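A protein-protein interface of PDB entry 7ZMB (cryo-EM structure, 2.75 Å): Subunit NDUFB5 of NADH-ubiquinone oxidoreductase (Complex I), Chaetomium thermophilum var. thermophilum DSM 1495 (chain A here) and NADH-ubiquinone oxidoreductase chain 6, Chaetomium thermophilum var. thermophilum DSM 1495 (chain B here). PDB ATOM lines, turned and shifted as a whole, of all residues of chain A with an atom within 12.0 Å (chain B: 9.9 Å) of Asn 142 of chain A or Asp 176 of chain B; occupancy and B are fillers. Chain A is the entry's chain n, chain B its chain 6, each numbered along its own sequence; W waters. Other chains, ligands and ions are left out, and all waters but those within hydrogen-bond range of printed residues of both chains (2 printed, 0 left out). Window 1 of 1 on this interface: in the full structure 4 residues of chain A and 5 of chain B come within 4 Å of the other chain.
Asn 142 of chain A touches Asp 176 of chain B (C to O, 3.7 Å). CA of Gly 177 of chain B touches O of Asn 142 of chain A (3.3 Å). Asn 142 of chain A touches Leu 179 of chain B (OD1 to N, 3.9 Å). Asn 142 of chain A touches Glu 181 of chain B. Val 143 of chain A touches Asp 176 of chain B (O to O, 3.8 Å). Pro 144 of chain A touches Asp 176 of chain B.
Printed residues of chain B within 4 Å of Asn 142 of chain A: Asp 176 (3.7 Å), Gly 177 (3.3 Å), Leu 179 (3.9 Å), Ala 180 (2.8 Å) and Glu 181 (3.8 Å). Of chain B, only Asp 176 comes within 4 Å of Val 143 of chain A. Of the printed residues of chain B, Pro 144 of chain A touches Asp 176 (3.6 Å). Of the printed residues of chain B, Ala 145 of chain A touches Asp 176 (3.3 Å). No residue of chain A comes within 4 Å of Ile 174 of chain B. Of chain A, only Asn 142 (3.7 Å), Val 143 (3.8 Å), Pro 144 (3.6 Å) and Ala 145 (3.3 Å) come within 4 Å of Asp 176 of chain B. Gly 177 of chain B touches just one residue of chain A: Asn 142 (3.3 Å). Printed residues of chain A within 4 Å of Leu 179 of chain B: Asn 142. Of the printed residues of chain A, Glu 181 of chain B touches Asn 142 (3.8 Å). The nearest printed residue of chain B that does not touch Asn 142 of chain A is Asn 182 of chain B (4.005 Å). The nearest residue of chain A that does not touch Asp 176 of chain B is Phe 141 of chain A (6.1 Å).
The backbone carbonyl oxygen of Ala 180 of chain B sits close to the side-chain amide oxygen of Asn 182 of chain B (2.8 Å).
Of the 11 printed residues of chain A, 4 touch a printed residue of chain B. Hydrophobic or aromatic side chains of chain A that line the printed part of chain B: Ala 145. Along chain A the printed residues that touch a printed residue of chain B span positions 142 to 145. Of the 14 printed residues of chain B, 5 touch a printed residue of chain A. Printed residues of chain B that touch a printed residue of chain A: Asp 176, Gly 177, Leu 179, Ala 180 and Glu 181.
ND2 of Asn 142 of chain A sits at hydrogen-bond distance from O of Ala 180 of chain B (2.8 Å). The side-chain carboxylate (OD2) of Asp 176 of chain B sits at hydrogen-bond distance from the backbone NH (N) of Ala 145 of chain A, 3.3 Å away.
Water W2 lies within hydrogen-bond range of the side-chain carboxylate of Asp 176 of chain B (2.6 Å) and the backbone NH of Ala 145 of chain A (3.0 Å). Water W1 lies within hydrogen-bond range of the backbone carbonyl oxygen of Asp 176 of chain B (2.6 Å) and the backbone carbonyl oxygen of Val 143 of chain A (3.5 Å).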
ATOM      1  N   GLY A 138      -0.301  14.297  -8.876  1.00  0.00           N
ATOM      2  CA  GLY A 138      -1.088  14.286 -10.124  1.00  0.00           C
ATOM      3  C   GLY A 138      -1.830  15.584 -10.332  1.00  0.00           C
ATOM      4  O   GLY A 138      -2.343  16.118  -9.348  1.00  0.00           O
ATOM      5  N   SER A 139      -1.917  16.048 -11.578  1.00  0.00           N
ATOM      6  CA  SER A 139      -2.580  17.342 -11.890  1.00  0.00           C
ATOM      7  C   SER A 139      -4.072  17.287 -11.572  1.00  0.00           C
ATOM      8  O   SER A 139      -4.693  16.261 -11.853  1.00  0.00           O
ATOM      9  CB  SER A 139      -2.350  17.726 -13.321  1.00  0.00           C
ATOM     10  OG  SER A 139      -2.857  19.023 -13.584  1.00  0.00           O
ATOM     11  N   PRO A 140      -4.674  18.356 -11.013  1.00  0.00           N
ATOM     12  CA  PRO A 140      -6.126  18.398 -10.788  1.00  0.00           C
ATOM     13  C   PRO A 140      -6.890  18.941 -12.003  1.00  0.00           C
ATOM     14  O   PRO A 140      -8.068  19.132 -11.894  1.00  0.00           O
ATOM     15  CB  PRO A 140      -6.218  19.370  -9.614  1.00  0.00           C
ATOM     16  CG  PRO A 140      -5.097  20.347  -9.853  1.00  0.00           C
ATOM     17  CD  PRO A 140      -3.985  19.527 -10.470  1.00  0.00           C
ATOM     18  N   PHE A 141      -6.202  19.186 -13.106  1.00  0.00           N
ATOM     19  CA  PHE A 141      -6.811  19.826 -14.295  1.00  0.00           C
ATOM     20  C   PHE A 141      -6.761  18.949 -15.530  1.00  0.00           C
ATOM     21  O   PHE A 141      -5.844  18.133 -15.623  1.00  0.00           O
ATOM     22  CB  PHE A 141      -6.012  21.072 -14.684  1.00  0.00           C
ATOM     23  CG  PHE A 141      -5.639  21.981 -13.545  1.00  0.00           C
ATOM     24  CD1 PHE A 141      -6.612  22.674 -12.848  1.00  0.00           C
ATOM     25  CD2 PHE A 141      -4.315  22.154 -13.186  1.00  0.00           C
ATOM     26  CE1 PHE A 141      -6.265  23.513 -11.805  1.00  0.00           C
ATOM     27  CE2 PHE A 141      -3.971  22.992 -12.138  1.00  0.00           C
ATOM     28  CZ  PHE A 141      -4.949  23.662 -11.445  1.00  0.00           C
ATOM     29  N   ASN A 142      -7.806  19.042 -16.355  1.00  0.00           N
ATOM     30  CA  ASN A 142      -7.855  18.329 -17.656  1.00  0.00           C
ATOM     31  C   ASN A 142      -7.773  16.831 -17.420  1.00  0.00           C
ATOM     32  O   ASN A 142      -7.114  16.142 -18.209  1.00  0.00           O
ATOM     33  CB  ASN A 142      -6.791  18.845 -18.623  1.00  0.00           C
ATOM     34  CG  ASN A 142      -6.951  20.298 -19.001  1.00  0.00           C
ATOM     35  OD1 ASN A 142      -8.036  20.858 -18.889  1.00  0.00           O
ATOM     36  ND2 ASN A 142      -5.870  20.905 -19.455  1.00  0.00           N
ATOM     37  N   VAL A 143      -8.433  16.357 -16.376  1.00  0.00           N
ATOM     38  CA  VAL A 143      -8.296  14.920 -16.034  1.00  0.00           C
ATOM     39  C   VAL A 143      -9.280  14.151 -16.903  1.00  0.00           C
ATOM     40  O   VAL A 143     -10.468  14.470 -16.869  1.00  0.00           O
ATOM     41  CB  VAL A 143      -8.484  14.674 -14.524  1.00  0.00           C
ATOM     42  CG1 VAL A 143      -8.455  13.198 -14.169  1.00  0.00           C
ATOM     43  CG2 VAL A 143      -7.475  15.454 -13.701  1.00  0.00           C
ATOM     44  N   PRO A 144      -8.818  13.163 -17.692  1.00  0.00           N
ATOM     45  CA  PRO A 144      -9.739  12.326 -18.456  1.00  0.00           C
ATOM     46  C   PRO A 144     -10.537  11.522 -17.423  1.00  0.00           C
ATOM     47  O   PRO A 144      -9.996  11.243 -16.387  1.00  0.00           O
ATOM     48  CB  PRO A 144      -8.792  11.464 -19.302  1.00  0.00           C
ATOM     49  CG  PRO A 144      -7.464  12.175 -19.262  1.00  0.00           C
ATOM     50  CD  PRO A 144      -7.415  12.822 -17.901  1.00  0.00           C
ATOM     51  N   ALA A 145     -11.799  11.202 -17.690  1.00  0.00           N
ATOM     52  CA  ALA A 145     -12.543  10.328 -16.748  1.00  0.00           C
ATOM     53  C   ALA A 145     -11.935   8.926 -16.732  1.00  0.00           C
ATOM     54  O   ALA A 145     -11.650   8.387 -17.814  1.00  0.00           O
ATOM     55  CB  ALA A 145     -14.001  10.275 -17.083  1.00  0.00           C
ATOM     56  N   GLY A 146     -11.763   8.359 -15.540  1.00  0.00           N
ATOM     57  CA  GLY A 146     -11.188   7.016 -15.393  1.00  0.00           C
ATOM     58  C   GLY A 146      -9.702   6.973 -15.647  1.00  0.00           C
ATOM     59  O   GLY A 146      -9.174   5.873 -15.836  1.00  0.00           O
ATOM     60  N   PHE A 147      -9.044   8.124 -15.639  1.00  0.00           N
ATOM     61  CA  PHE A 147      -7.573   8.137 -15.822  1.00  0.00           C
ATOM     62  C   PHE A 147      -6.862   7.639 -14.558  1.00  0.00           C
ATOM     63  O   PHE A 147      -6.028   6.730 -14.654  1.00  0.00           O
ATOM     64  CB  PHE A 147      -7.121   9.533 -16.244  1.00  0.00           C
ATOM     65  CG  PHE A 147      -5.634   9.760 -16.204  1.00  0.00           C
ATOM     66  CD1 PHE A 147      -5.004  10.118 -15.023  1.00  0.00           C
ATOM     67  CD2 PHE A 147      -4.872   9.638 -17.352  1.00  0.00           C
ATOM     68  CE1 PHE A 147      -3.637  10.309 -14.980  1.00  0.00           C
ATOM     69  CE2 PHE A 147      -3.506   9.855 -17.313  1.00  0.00           C
ATOM     70  CZ  PHE A 147      -2.897  10.193 -16.129  1.00  0.00           C
ATOM     71  N   TYR A 148      -7.254   8.153 -13.400  1.00  0.00           N
ATOM     72  CA  TYR A 148      -6.531   7.818 -12.147  1.00  0.00           C
ATOM     73  C   TYR A 148      -6.923   6.423 -11.647  1.00  0.00           C
ATOM     74  O   TYR A 148      -8.115   6.084 -11.712  1.00  0.00           O
ATOM     75  CB  TYR A 148      -6.778   8.855 -11.052  1.00  0.00           C
ATOM     76  CG  TYR A 148      -6.032  10.153 -11.219  1.00  0.00           C
ATOM     77  CD1 TYR A 148      -4.653  10.201 -11.130  1.00  0.00           C
ATOM     78  CD2 TYR A 148      -6.708  11.337 -11.450  1.00  0.00           C
ATOM     79  CE1 TYR A 148      -3.963  11.390 -11.284  1.00  0.00           C
ATOM     80  CE2 TYR A 148      -6.035  12.535 -11.601  1.00  0.00           C
ATOM     81  CZ  TYR A 148      -4.656  12.561 -11.523  1.00  0.00           C
ATOM     82  OH  TYR A 148      -3.987  13.736 -11.681  1.00  0.00           O
ATOM     83  N   LYS B 173      -8.025  12.230 -30.679  1.00  0.00           N
ATOM     84  CA  LYS B 173      -8.422  13.383 -29.840  1.00  0.00           C
ATOM     85  C   LYS B 173      -9.172  12.933 -28.588  1.00  0.00           C
ATOM     86  O   LYS B 173      -9.770  11.857 -28.635  1.00  0.00           O
ATOM     87  CB  LYS B 173      -9.279  14.308 -30.704  1.00  0.00           C
ATOM     88  CG  LYS B 173     -10.654  13.781 -31.083  1.00  0.00           C
ATOM     89  CD  LYS B 173     -11.479  14.769 -31.862  1.00  0.00           C
ATOM     90  CE  LYS B 173     -10.888  15.119 -33.210  1.00  0.00           C
ATOM     91  NZ  LYS B 173     -11.759  16.063 -33.949  1.00  0.00           N
ATOM     92  N   ILE B 174      -9.088  13.695 -27.497  1.00  0.00           N
ATOM     93  CA  ILE B 174      -9.939  13.430 -26.300  1.00  0.00           C
ATOM     94  C   ILE B 174     -10.613  14.761 -25.987  1.00  0.00           C
ATOM     95  O   ILE B 174     -10.157  15.778 -26.515  1.00  0.00           O
ATOM     96  CB  ILE B 174      -9.187  12.873 -25.069  1.00  0.00           C
ATOM     97  CG1 ILE B 174      -7.983  13.733 -24.679  1.00  0.00           C
ATOM     98  CG2 ILE B 174      -8.818  11.410 -25.253  1.00  0.00           C
ATOM     99  CD1 ILE B 174      -7.357  13.333 -23.365  1.00  0.00           C
ATOM    100  N   TRP B 175     -11.688  14.737 -25.212  1.00  0.00           N
ATOM    101  CA  TRP B 175     -12.429  15.968 -24.853  1.00  0.00           C
ATOM    102  C   TRP B 175     -12.271  16.276 -23.363  1.00  0.00           C
ATOM    103  O   TRP B 175     -12.206  17.460 -23.018  1.00  0.00           O
ATOM    104  CB  TRP B 175     -13.886  15.771 -25.272  1.00  0.00           C
ATOM    105  CG  TRP B 175     -14.017  15.582 -26.752  1.00  0.00           C
ATOM    106  CD1 TRP B 175     -14.134  14.402 -27.425  1.00  0.00           C
ATOM    107  CD2 TRP B 175     -14.009  16.613 -27.755  1.00  0.00           C
ATOM    108  NE1 TRP B 175     -14.216  14.627 -28.770  1.00  0.00           N
ATOM    109  CE2 TRP B 175     -14.143  15.974 -29.006  1.00  0.00           C
ATOM    110  CE3 TRP B 175     -13.916  18.009 -27.721  1.00  0.00           C
ATOM    111  CZ2 TRP B 175     -14.183  16.681 -30.205  1.00  0.00           C
ATOM    112  CZ3 TRP B 175     -13.952  18.708 -28.906  1.00  0.00           C
ATOM    113  CH2 TRP B 175     -14.090  18.051 -30.129  1.00  0.00           C
ATOM    114  N   ASP B 176     -12.182  15.248 -22.525  1.00  0.00           N
ATOM    115  CA  ASP B 176     -12.045  15.425 -21.054  1.00  0.00           C
ATOM    116  C   ASP B 176     -10.693  16.072 -20.741  1.00  0.00           C
ATOM    117  O   ASP B 176     -10.630  16.879 -19.811  1.00  0.00           O
ATOM    118  CB  ASP B 176     -12.280  14.121 -20.294  1.00  0.00           C
ATOM    119  CG  ASP B 176     -13.537  13.374 -20.696  1.00  0.00           C
ATOM    120  OD1 ASP B 176     -14.134  13.735 -21.720  1.00  0.00           O
ATOM    121  OD2 ASP B 176     -13.910  12.433 -19.977  1.00  0.00           O
ATOM    122  N   GLY B 177      -9.656  15.717 -21.493  1.00  0.00           N
ATOM    123  CA  GLY B 177      -8.315  16.294 -21.300  1.00  0.00           C
ATOM    124  C   GLY B 177      -8.118  17.557 -22.108  1.00  0.00           C
ATOM    125  O   GLY B 177      -7.006  18.083 -22.096  1.00  0.00           O
ATOM    126  N   ALA B 178      -9.160  18.006 -22.802  1.00  0.00           N
ATOM    127  CA  ALA B 178      -9.075  19.248 -23.601  1.00  0.00           C
ATOM    128  C   ALA B 178      -9.962  20.355 -23.031  1.00  0.00           C
ATOM    129  O   ALA B 178     -10.104  21.379 -23.723  1.00  0.00           O
ATOM    130  CB  ALA B 178      -9.448  18.964 -25.026  1.00  0.00           C
ATOM    131  N   LEU B 179     -10.538  20.178 -21.839  1.00  0.00           N
ATOM    132  CA  LEU B 179     -11.479  21.221 -21.366  1.00  0.00           C
ATOM    133  C   LEU B 179     -10.766  22.574 -21.258  1.00  0.00           C
ATOM    134  O   LEU B 179     -11.318  23.560 -21.748  1.00  0.00           O
ATOM    135  CB  LEU B 179     -12.056  20.793 -20.014  1.00  0.00           C
ATOM    136  CG  LEU B 179     -12.863  21.866 -19.286  1.00  0.00           C
ATOM    137  CD1 LEU B 179     -14.164  22.154 -20.011  1.00  0.00           C
ATOM    138  CD2 LEU B 179     -13.140  21.456 -17.855  1.00  0.00           C
ATOM    139  N   ALA B 180      -9.594  22.628 -20.630  1.00  0.00           N
ATOM    140  CA  ALA B 180      -8.798  23.875 -20.609  1.00  0.00           C
ATOM    141  C   ALA B 180      -7.334  23.574 -20.942  1.00  0.00           C
ATOM    142  O   ALA B 180      -6.532  23.595 -20.013  1.00  0.00           O
ATOM    143  CB  ALA B 180      -8.921  24.533 -19.269  1.00  0.00           C
ATOM    144  N   GLU B 181      -7.012  23.348 -22.242  1.00  0.00           N
ATOM    145  CA  GLU B 181      -5.607  22.997 -22.578  1.00  0.00           C
ATOM    146  C   GLU B 181      -4.702  24.176 -22.220  1.00  0.00           C
ATOM    147  O   GLU B 181      -5.007  25.303 -22.646  1.00  0.00           O
ATOM    148  CB  GLU B 181      -5.455  22.590 -24.042  1.00  0.00           C
ATOM    149  CG  GLU B 181      -4.016  22.490 -24.513  1.00  0.00           C
ATOM    150  CD  GLU B 181      -3.642  23.493 -25.591  1.00  0.00           C
ATOM    151  OE1 GLU B 181      -4.559  24.042 -26.228  1.00  0.00           O
ATOM    152  OE2 GLU B 181      -2.434  23.732 -25.781  1.00  0.00           O
ATOM    153  N   ASN B 182      -3.627  23.896 -21.419  1.00  0.00           N
ATOM    154  CA  ASN B 182      -2.705  24.994 -21.039  1.00  0.00           C
ATOM    155  C   ASN B 182      -1.540  25.049 -22.023  1.00  0.00           C
ATOM    156  O   ASN B 182      -1.346  24.062 -22.738  1.00  0.00           O
ATOM    157  CB  ASN B 182      -2.136  24.810 -19.629  1.00  0.00           C
ATOM    158  CG  ASN B 182      -3.137  24.980 -18.510  1.00  0.00           C
ATOM    159  OD1 ASN B 182      -4.241  24.454 -18.567  1.00  0.00           O
ATOM    160  ND2 ASN B 182      -2.739  25.685 -17.468  1.00  0.00           N
ATOM    161  N   ASN B 183      -0.803  26.157 -22.057  1.00  0.00           N
ATOM    162  CA  ASN B 183       0.440  26.191 -22.868  1.00  0.00           C
ATOM    163  C   ASN B 183       1.562  25.653 -21.991  1.00  0.00           C
ATOM    164  O   ASN B 183       1.412  25.707 -20.776  1.00  0.00           O
ATOM    165  CB  ASN B 183       0.727  27.600 -23.392  1.00  0.00           C
ATOM    166  CG  ASN B 183      -0.452  28.220 -24.103  1.00  0.00           C
ATOM    167  OD1 ASN B 183      -1.068  27.589 -24.957  1.00  0.00           O
ATOM    168  ND2 ASN B 183      -0.772  29.457 -23.764  1.00  0.00           N
ATOM    169  N   SER B 186       2.546  27.657 -19.122  1.00  0.00           N
ATOM    170  CA  SER B 186       1.562  27.646 -18.013  1.00  0.00           C
ATOM    171  C   SER B 186       1.611  26.309 -17.256  1.00  0.00           C
ATOM    172  O   SER B 186       1.467  26.335 -16.034  1.00  0.00           O
ATOM    173  CB  SER B 186       0.191  27.987 -18.529  1.00  0.00           C
ATOM    174  OG  SER B 186      -0.732  28.104 -17.458  1.00  0.00           O
ATOM    175  N   SER B 187       1.846  25.197 -17.946  1.00  0.00           N
ATOM    176  CA  SER B 187       1.919  23.859 -17.308  1.00  0.00           C
ATOM    177  C   SER B 187       3.087  23.821 -16.334  1.00  0.00           C
ATOM    178  O   SER B 187       2.965  23.182 -15.278  1.00  0.00           O
ATOM    179  CB  SER B 187       2.016  22.765 -18.309  1.00  0.00           C
ATOM    180  OG  SER B 187       1.078  22.967 -19.350  1.00  0.00           O
ATOM    181  N   ASN B 190       2.191  26.063 -13.416  1.00  0.00           N
ATOM    182  CA  ASN B 190       1.237  25.424 -12.519  1.00  0.00           C
ATOM    183  C   ASN B 190       1.917  24.683 -11.379  1.00  0.00           C
ATOM    184  O   ASN B 190       1.268  24.399 -10.370  1.00  0.00           O
ATOM    185  CB  ASN B 190       0.346  24.461 -13.300  1.00  0.00           C
ATOM    186  CG  ASN B 190      -0.739  25.170 -14.090  1.00  0.00           C
ATOM    187  OD1 ASN B 190      -1.052  26.330 -13.841  1.00  0.00           O
ATOM    188  ND2 ASN B 190      -1.315  24.468 -15.056  1.00  0.00           N
HETATM  189  O   HOH W   1     -11.928  17.508 -17.631  1.00  0.00           O
HETATM  190  O   HOH W   2     -12.587  10.210 -20.355  1.00  0.00           O
